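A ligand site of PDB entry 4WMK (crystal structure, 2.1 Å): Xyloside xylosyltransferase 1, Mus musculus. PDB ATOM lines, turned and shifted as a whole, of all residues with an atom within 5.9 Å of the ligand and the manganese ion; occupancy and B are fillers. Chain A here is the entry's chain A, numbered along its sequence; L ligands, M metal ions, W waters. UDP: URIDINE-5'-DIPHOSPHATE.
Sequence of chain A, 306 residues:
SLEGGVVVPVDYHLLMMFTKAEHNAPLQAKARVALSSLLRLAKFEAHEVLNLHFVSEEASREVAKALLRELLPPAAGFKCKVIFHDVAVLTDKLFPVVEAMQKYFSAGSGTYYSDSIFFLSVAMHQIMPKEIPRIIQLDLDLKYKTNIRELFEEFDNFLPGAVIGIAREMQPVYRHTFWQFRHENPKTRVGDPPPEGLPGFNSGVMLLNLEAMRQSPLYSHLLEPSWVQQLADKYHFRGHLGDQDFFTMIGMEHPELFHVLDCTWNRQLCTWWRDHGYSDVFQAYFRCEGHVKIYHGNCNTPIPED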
ATOM      1  N   MET A  16     -15.585   7.577  10.758  1.00  0.00           N
ATOM      2  CA  MET A  16     -14.273   7.196  10.234  1.00  0.00           C
ATOM      3  C   MET A  16     -13.190   7.264  11.300  1.00  0.00           C
ATOM      4  O   MET A  16     -13.145   8.227  12.099  1.00  0.00           O
ATOM      5  CB  MET A  16     -13.909   8.105   9.050  1.00  0.00           C
ATOM      6  CG  MET A  16     -14.850   7.904   7.861  1.00  0.00           C
ATOM      7  SD  MET A  16     -14.841   9.260   6.702  1.00  0.00           S
ATOM      8  CE  MET A  16     -16.517   9.236   6.081  1.00  0.00           C
ATOM      9  N   MET A  17     -12.325   6.249  11.304  1.00  0.00           N
ATOM     10  CA  MET A  17     -11.076   6.220  12.074  1.00  0.00           C
ATOM     11  C   MET A  17     -10.032   7.054  11.385  1.00  0.00           C
ATOM     12  O   MET A  17      -9.804   6.898  10.200  1.00  0.00           O
ATOM     13  CB  MET A  17     -10.514   4.805  12.148  1.00  0.00           C
ATOM     14  CG  MET A  17     -11.424   3.800  12.809  1.00  0.00           C
ATOM     15  SD  MET A  17     -11.549   4.267  14.548  1.00  0.00           S
ATOM     16  CE  MET A  17      -9.794   4.156  14.988  1.00  0.00           C
ATOM     17  N   PHE A  18      -9.391   7.943  12.130  1.00  0.00           N
ATOM     18  CA  PHE A  18      -8.388   8.811  11.538  1.00  0.00           C
ATOM     19  C   PHE A  18      -7.388   9.115  12.613  1.00  0.00           C
ATOM     20  O   PHE A  18      -7.509  10.142  13.318  1.00  0.00           O
ATOM     21  CB  PHE A  18      -9.007  10.106  10.972  1.00  0.00           C
ATOM     22  CG  PHE A  18      -8.052  10.939  10.147  1.00  0.00           C
ATOM     23  CD1 PHE A  18      -7.475  10.430   8.968  1.00  0.00           C
ATOM     24  CD2 PHE A  18      -7.710  12.221  10.545  1.00  0.00           C
ATOM     25  CE1 PHE A  18      -6.600  11.184   8.204  1.00  0.00           C
ATOM     26  CE2 PHE A  18      -6.838  13.007   9.777  1.00  0.00           C
ATOM     27  CZ  PHE A  18      -6.289  12.486   8.605  1.00  0.00           C
ATOM     28  N   THR A  19      -6.422   8.225  12.756  1.00  0.00           N
ATOM     29  CA  THR A  19      -5.465   8.284  13.837  1.00  0.00           C
ATOM     30  C   THR A  19      -4.041   8.243  13.281  1.00  0.00           C
ATOM     31  O   THR A  19      -3.802   7.699  12.185  1.00  0.00           O
ATOM     32  CB  THR A  19      -5.637   7.103  14.805  1.00  0.00           C
ATOM     33  OG1 THR A  19      -5.519   5.881  14.062  1.00  0.00           O
ATOM     34  CG2 THR A  19      -7.003   7.142  15.504  1.00  0.00           C
ATOM     35  N   LYS A  20      -3.101   8.779  14.072  1.00  0.00           N
ATOM     36  CA  LYS A  20      -1.675   8.755  13.745  1.00  0.00           C
ATOM     37  C   LYS A  20      -1.446   9.342  12.356  1.00  0.00           C
ATOM     38  O   LYS A  20      -0.616   8.852  11.590  1.00  0.00           O
ATOM     39  CB  LYS A  20      -1.106   7.331  13.841  1.00  0.00           C
ATOM     40  CG  LYS A  20      -1.410   6.575  15.122  1.00  0.00           C
ATOM     41  CD  LYS A  20      -0.700   7.156  16.326  1.00  0.00           C
ATOM     42  CE  LYS A  20      -0.781   6.235  17.527  1.00  0.00           C
ATOM     43  NZ  LYS A  20      -0.430   4.829  17.170  1.00  0.00           N
ATOM     44  N   ALA A  21      -2.177  10.410  12.030  1.00  0.00           N
ATOM     45  CA  ALA A  21      -2.165  10.991  10.695  1.00  0.00           C
ATOM     46  C   ALA A  21      -1.080  12.069  10.480  1.00  0.00           C
ATOM     47  O   ALA A  21      -0.726  12.365   9.339  1.00  0.00           O
ATOM     48  CB  ALA A  21      -3.527  11.548  10.333  1.00  0.00           C
ATOM     49  N   ASN A  24       2.038  11.370   8.235  1.00  0.00           N
ATOM     50  CA  ASN A  24       1.651  10.164   7.530  1.00  0.00           C
ATOM     51  C   ASN A  24       0.935  10.591   6.267  1.00  0.00           C
ATOM     52  O   ASN A  24      -0.295  10.598   6.205  1.00  0.00           O
ATOM     53  CB  ASN A  24       0.780   9.246   8.407  1.00  0.00           C
ATOM     54  CG  ASN A  24       0.468   7.929   7.742  1.00  0.00           C
ATOM     55  OD1 ASN A  24       0.682   7.756   6.545  1.00  0.00           O
ATOM     56  ND2 ASN A  24      -0.056   6.985   8.509  1.00  0.00           N
ATOM     57  N   LEU A  27      -1.660   8.307   4.368  1.00  0.00           N
ATOM     58  CA  LEU A  27      -2.985   8.322   4.978  1.00  0.00           C
ATOM     59  C   LEU A  27      -3.750   9.613   4.729  1.00  0.00           C
ATOM     60  O   LEU A  27      -4.950   9.575   4.413  1.00  0.00           O
ATOM     61  CB  LEU A  27      -2.898   7.995   6.495  1.00  0.00           C
ATOM     62  CG  LEU A  27      -4.149   8.067   7.390  1.00  0.00           C
ATOM     63  CD1 LEU A  27      -5.181   6.992   7.070  1.00  0.00           C
ATOM     64  CD2 LEU A  27      -3.742   7.939   8.847  1.00  0.00           C
ATOM     65  N   LYS A  30      -5.040   9.447   1.146  1.00  0.00           N
ATOM     66  CA  LYS A  30      -6.182   8.535   1.171  1.00  0.00           C
ATOM     67  C   LYS A  30      -7.420   9.251   1.699  1.00  0.00           C
ATOM     68  O   LYS A  30      -8.486   9.222   1.071  1.00  0.00           O
ATOM     69  CB  LYS A  30      -5.876   7.307   2.041  1.00  0.00           C
ATOM     70  CG  LYS A  30      -5.007   6.268   1.358  1.00  0.00           C
ATOM     71  CD  LYS A  30      -4.558   5.269   2.403  1.00  0.00           C
ATOM     72  CE  LYS A  30      -3.822   4.107   1.786  1.00  0.00           C
ATOM     73  NZ  LYS A  30      -3.565   3.092   2.838  1.00  0.00           N
ATOM     74  N   VAL A  55     -12.757   9.482  14.747  1.00  0.00           N
ATOM     75  CA  VAL A  55     -12.027   8.988  15.911  1.00  0.00           C
ATOM     76  C   VAL A  55     -10.532   9.250  15.683  1.00  0.00           C
ATOM     77  O   VAL A  55      -9.922   8.683  14.766  1.00  0.00           O
ATOM     78  CB  VAL A  55     -12.323   7.491  16.175  1.00  0.00           C
ATOM     79  CG1 VAL A  55     -11.641   7.006  17.446  1.00  0.00           C
ATOM     80  CG2 VAL A  55     -13.816   7.265  16.276  1.00  0.00           C
ATOM     81  N   PHE A 118      -9.499  -1.094  17.340  1.00  0.00           N
ATOM     82  CA  PHE A 118      -9.850  -1.871  16.125  1.00  0.00           C
ATOM     83  C   PHE A 118     -11.131  -2.716  16.331  1.00  0.00           C
ATOM     84  O   PHE A 118     -11.635  -3.315  15.388  1.00  0.00           O
ATOM     85  CB  PHE A 118      -8.632  -2.682  15.581  1.00  0.00           C
ATOM     86  CG  PHE A 118      -7.438  -1.816  15.256  1.00  0.00           C
ATOM     87  CD1 PHE A 118      -7.523  -0.818  14.262  1.00  0.00           C
ATOM     88  CD2 PHE A 118      -6.243  -1.941  15.960  1.00  0.00           C
ATOM     89  CE1 PHE A 118      -6.428   0.027  13.986  1.00  0.00           C
ATOM     90  CE2 PHE A 118      -5.138  -1.124  15.661  1.00  0.00           C
ATOM     91  CZ  PHE A 118      -5.233  -0.131  14.685  1.00  0.00           C
ATOM     92  N   LEU A 138     -16.870   3.749   7.974  1.00  0.00           N
ATOM     93  CA  LEU A 138     -16.193   3.675   6.692  1.00  0.00           C
ATOM     94  C   LEU A 138     -14.688   3.845   6.841  1.00  0.00           C
ATOM     95  O   LEU A 138     -14.233   4.677   7.634  1.00  0.00           O
ATOM     96  CB  LEU A 138     -16.729   4.776   5.757  1.00  0.00           C
ATOM     97  CG  LEU A 138     -18.242   4.811   5.498  1.00  0.00           C
ATOM     98  CD1 LEU A 138     -18.715   6.226   5.174  1.00  0.00           C
ATOM     99  CD2 LEU A 138     -18.628   3.831   4.405  1.00  0.00           C
ATOM    100  N   ASP A 139     -13.914   3.060   6.088  1.00  0.00           N
ATOM    101  CA  ASP A 139     -12.461   3.281   5.963  1.00  0.00           C
ATOM    102  C   ASP A 139     -12.161   4.596   5.256  1.00  0.00           C
ATOM    103  O   ASP A 139     -13.049   5.195   4.616  1.00  0.00           O
ATOM    104  CB  ASP A 139     -11.803   2.145   5.187  1.00  0.00           C
ATOM    105  CG  ASP A 139     -11.535   0.923   6.042  1.00  0.00           C
ATOM    106  OD1 ASP A 139     -12.060   0.859   7.174  1.00  0.00           O
ATOM    107  OD2 ASP A 139     -10.817   0.010   5.582  1.00  0.00           O
ATOM    108  N   LEU A 140     -10.917   5.049   5.353  1.00  0.00           N
ATOM    109  CA  LEU A 140     -10.509   6.257   4.642  1.00  0.00           C
ATOM    110  C   LEU A 140      -9.737   5.973   3.327  1.00  0.00           C
ATOM    111  O   LEU A 140      -9.357   6.899   2.622  1.00  0.00           O
ATOM    112  CB  LEU A 140      -9.764   7.228   5.579  1.00  0.00           C
ATOM    113  CG  LEU A 140     -10.742   8.087   6.421  1.00  0.00           C
ATOM    114  CD1 LEU A 140     -10.070   8.838   7.564  1.00  0.00           C
ATOM    115  CD2 LEU A 140     -11.527   9.050   5.540  1.00  0.00           C
ATOM    116  N   ASP A 141      -9.532   4.701   3.013  1.00  0.00           N
ATOM    117  CA  ASP A 141      -8.899   4.327   1.738  1.00  0.00           C
ATOM    118  C   ASP A 141      -9.978   3.912   0.720  1.00  0.00           C
ATOM    119  O   ASP A 141      -9.841   2.914   0.000  1.00  0.00           O
ATOM    120  CB  ASP A 141      -7.861   3.226   1.966  1.00  0.00           C
ATOM    121  CG  ASP A 141      -8.450   1.955   2.571  1.00  0.00           C
ATOM    122  OD1 ASP A 141      -9.519   2.024   3.200  1.00  0.00           O
ATOM    123  OD2 ASP A 141      -7.837   0.882   2.427  1.00  0.00           O
ATOM    124  N   LEU A 142     -11.057   4.709   0.673  1.00  0.00           N
ATOM    125  CA  LEU A 142     -12.195   4.494  -0.225  1.00  0.00           C
ATOM    126  C   LEU A 142     -12.303   5.571  -1.281  1.00  0.00           C
ATOM    127  O   LEU A 142     -11.736   6.661  -1.133  1.00  0.00           O
ATOM    128  CB  LEU A 142     -13.509   4.477   0.573  1.00  0.00           C
ATOM    129  CG  LEU A 142     -13.668   3.417   1.661  1.00  0.00           C
ATOM    130  CD1 LEU A 142     -15.002   3.535   2.383  1.00  0.00           C
ATOM    131  CD2 LEU A 142     -13.510   2.024   1.059  1.00  0.00           C
ATOM    132  N   GLY A 204     -14.543  -2.571   5.712  1.00  0.00           N
ATOM    133  CA  GLY A 204     -14.342  -1.257   5.107  1.00  0.00           C
ATOM    134  C   GLY A 204     -15.579  -0.375   5.050  1.00  0.00           C
ATOM    135  O   GLY A 204     -15.453   0.839   5.037  1.00  0.00           O
ATOM    136  N   LEU A 241      -7.056  -8.870  12.407  1.00  0.00           N
ATOM    137  CA  LEU A 241      -7.828  -7.873  11.664  1.00  0.00           C
ATOM    138  C   LEU A 241      -9.003  -7.278  12.439  1.00  0.00           C
ATOM    139  O   LEU A 241      -9.799  -6.523  11.866  1.00  0.00           O
ATOM    140  CB  LEU A 241      -8.280  -8.417  10.293  1.00  0.00           C
ATOM    141  CG  LEU A 241      -7.166  -8.805   9.332  1.00  0.00           C
ATOM    142  CD1 LEU A 241      -7.720  -9.328   8.015  1.00  0.00           C
ATOM    143  CD2 LEU A 241      -6.226  -7.614   9.106  1.00  0.00           C
ATOM    144  N   HIS A 296     -12.605   0.289  -2.784  1.00  0.00           N
ATOM    145  CA  HIS A 296     -11.841   0.165  -1.554  1.00  0.00           C
ATOM    146  C   HIS A 296     -10.431  -0.245  -1.872  1.00  0.00           C
ATOM    147  O   HIS A 296     -10.150  -1.399  -2.207  1.00  0.00           O
ATOM    148  CB  HIS A 296     -12.559  -0.830  -0.654  1.00  0.00           C
ATOM    149  CG  HIS A 296     -11.959  -0.994   0.725  1.00  0.00           C
ATOM    150  ND1 HIS A 296     -12.397  -1.936   1.583  1.00  0.00           N
ATOM    151  CD2 HIS A 296     -10.917  -0.325   1.370  1.00  0.00           C
ATOM    152  CE1 HIS A 296     -11.688  -1.853   2.730  1.00  0.00           C
ATOM    153  NE2 HIS A 296     -10.779  -0.873   2.589  1.00  0.00           N
ATOM    154  N   GLY A 297      -9.523   0.729  -1.787  1.00  0.00           N
ATOM    155  CA  GLY A 297      -8.116   0.512  -2.097  1.00  0.00           C
ATOM    156  C   GLY A 297      -7.369  -0.158  -0.964  1.00  0.00           C
ATOM    157  O   GLY A 297      -6.338   0.370  -0.505  1.00  0.00           O
ATOM    158  N   ASN A 298      -7.869  -1.312  -0.493  1.00  0.00           N
ATOM    159  CA  ASN A 298      -7.219  -1.927   0.683  1.00  0.00           C
ATOM    160  C   ASN A 298      -5.796  -2.441   0.393  1.00  0.00           C
ATOM    161  O   ASN A 298      -5.382  -2.477  -0.759  1.00  0.00           O
ATOM    162  CB  ASN A 298      -8.115  -2.929   1.464  1.00  0.00           C
ATOM    163  CG  ASN A 298      -8.658  -4.077   0.601  1.00  0.00           C
ATOM    164  OD1 ASN A 298      -8.978  -5.136   1.137  1.00  0.00           O
ATOM    165  ND2 ASN A 298      -8.787  -3.870  -0.691  1.00  0.00           N
ATOM    166  N   CYS A 299      -5.065  -2.791   1.443  1.00  0.00           N
ATOM    167  CA  CYS A 299      -3.610  -3.047   1.372  1.00  0.00           C
ATOM    168  C   CYS A 299      -2.861  -2.039   0.486  1.00  0.00           C
ATOM    169  O   CYS A 299      -2.022  -2.394  -0.349  1.00  0.00           O
ATOM    170  CB  CYS A 299      -3.273  -4.536   1.075  1.00  0.00           C
ATOM    171  SG  CYS A 299      -3.439  -5.137  -0.633  1.00  0.00           S
ATOM    172  N   ASN A 300      -3.171  -0.764   0.684  1.00  0.00           N
ATOM    173  CA  ASN A 300      -2.490   0.319  -0.004  1.00  0.00           C
ATOM    174  C   ASN A 300      -2.580   0.179  -1.525  1.00  0.00           C
ATOM    175  O   ASN A 300      -1.684   0.605  -2.242  1.00  0.00           O
ATOM    176  CB  ASN A 300      -1.026   0.367   0.429  1.00  0.00           C
ATOM    177  CG  ASN A 300      -0.880   0.597   1.900  1.00  0.00           C
ATOM    178  OD1 ASN A 300      -1.469   1.508   2.439  1.00  0.00           O
ATOM    179  ND2 ASN A 300      -0.115  -0.228   2.552  1.00  0.00           N
HETATM  180  N1  UDP L   1      -6.421   3.947  10.037  1.00  0.00           N
HETATM  181  C2  UDP L   1      -5.977   5.159  10.639  1.00  0.00           C
HETATM  182  N3  UDP L   1      -4.689   5.332  10.945  1.00  0.00           N
HETATM  183  C4  UDP L   1      -3.799   4.366  10.691  1.00  0.00           C
HETATM  184  C5  UDP L   1      -4.177   3.161  10.098  1.00  0.00           C
HETATM  185  C6  UDP L   1      -5.524   2.963   9.783  1.00  0.00           C
HETATM  186  O2  UDP L   1      -6.798   6.066  10.901  1.00  0.00           O
HETATM  187  O4  UDP L   1      -2.610   4.585  10.975  1.00  0.00           O
HETATM  188  C1' UDP L   1      -7.851   3.801   9.747  1.00  0.00           C
HETATM  189  C2' UDP L   1      -8.170   4.364   8.381  1.00  0.00           C
HETATM  190  O2' UDP L   1      -9.475   4.955   8.436  1.00  0.00           O
HETATM  191  C3' UDP L   1      -8.204   3.125   7.494  1.00  0.00           C
HETATM  192  C4' UDP L   1      -8.632   1.990   8.435  1.00  0.00           C
HETATM  193  O4' UDP L   1      -8.261   2.426   9.745  1.00  0.00           O
HETATM  194  O3' UDP L   1      -9.085   3.328   6.373  1.00  0.00           O
HETATM  195  C5' UDP L   1      -7.942   0.637   8.201  1.00  0.00           C
HETATM  196  O5' UDP L   1      -6.653   0.801   7.597  1.00  0.00           O
HETATM  197  PA  UDP L   1      -6.532   0.741   5.985  1.00  0.00           P
HETATM  198  O1A UDP L   1      -5.411   1.624   5.464  1.00  0.00           O
HETATM  199  O2A UDP L   1      -7.926   1.028   5.454  1.00  0.00           O
HETATM  200  O3A UDP L   1      -6.117  -0.782   5.745  1.00  0.00           O
HETATM  201  PB  UDP L   1      -6.989  -1.919   5.008  1.00  0.00           P
HETATM  202  O1B UDP L   1      -6.024  -2.664   4.126  1.00  0.00           O
HETATM  203  O2B UDP L   1      -7.352  -2.667   6.263  1.00  0.00           O
HETATM  204  O3B UDP L   1      -8.183  -1.296   4.327  1.00  0.00           O
HETATM  205 MN    MN M   1      -9.441   0.041   3.998  1.00  0.00          MN
HETATM  206  O   HOH W   1      -5.149   0.838   2.335  1.00  0.00           O
HETATM  207  O   HOH W   2     -12.393   4.236   9.606  1.00  0.00           O
HETATM  208  O   HOH W   3      -3.516  -2.170   4.618  1.00  0.00           O
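Water W2 lies within hydrogen-bond range of N of Met 17 (2.6 Å), O of Leu 138 (2.7 Å) and O2' of the ligand (3.2 Å).
Water W1 lies within hydrogen-bond range of NZ of Lys 30 (2.8 Å), N of Asn 300 (3.0 Å), O of Gly 297 (3.1 Å) and O1A of the ligand (3.2 Å).
Within 4 Å of the manganese ion: Asp 139, Asp 141 and His 296.
The nearest printed residue that does not touch the manganese ion is Asn 298 (4.1 Å).
O1B of the ligand sits at hydrogen-bond distance from N of Cys 299 (2.9 Å).
The side-chain amino group of Lys 30 lies within salt-bridge range of an oxygen (O1A) of the ligand, 3.5 Å away.
A nitrogen (N3) of the ligand is in hydrogen-bond range of the side-chain hydroxyl of Thr 19 (3.3 Å).
The backbone NH (N) of Leu 140 sits at hydrogen-bond distance from an oxygen (O3') of the ligand (2.7 Å).
A nitrogen (N3) of the ligand is in hydrogen-bond range of the backbone carbonyl oxygen (O) of Thr 19, at 2.8 Å.
O of Met 17 lies within hydrogen-bond range of O2' of the ligand.
N of Thr 19 lies within hydrogen-bond range of O2 of the ligand.
O2 of the ligand sits close to N of Phe 18, at 3.4 Å.
Leu 27 touches the ligand (CD2 to N3, 3.5 Å).
CB of Asn 298 touches O3B of the ligand (3.3 Å).
Of the 23 residues printed, 11 come within 4 Å of the ligand.
The nearest printed residue that does not touch the ligand is Lys 20 (4.2 Å).
The manganese ion is bound by O3B of the ligand (1.9 Å), OD2 of Asp 139 (2.1 Å), OD1 of Asp 141 (2.1 Å), NE2 of His 296 (2.1 Å), O2A of the ligand (2.3 Å) and OD2 of Asp 141 (2.4 Å).
The manganese ion has six donor atoms within binding distance.
O of His 296 lies within hydrogen-bond range of ND2 of Asn 298 (3.2 Å).
O of Asp 141 sits at hydrogen-bond distance from N of Gly 297, 2.8 Å away.
The backbone NH (N) of Phe 18 lies within hydrogen-bond range of the backbone carbonyl oxygen (O) of Val 55 (2.8 Å).
N of Leu 27 lies within hydrogen-bond range of OD1 of Asn 24 (3.2 Å).
OD1 of Asn 300 sits at hydrogen-bond distance from NZ of Lys 30 (2.7 Å).
O of Gly 204 lies within hydrogen-bond range of N of Asp 139, at 2.9 Å.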
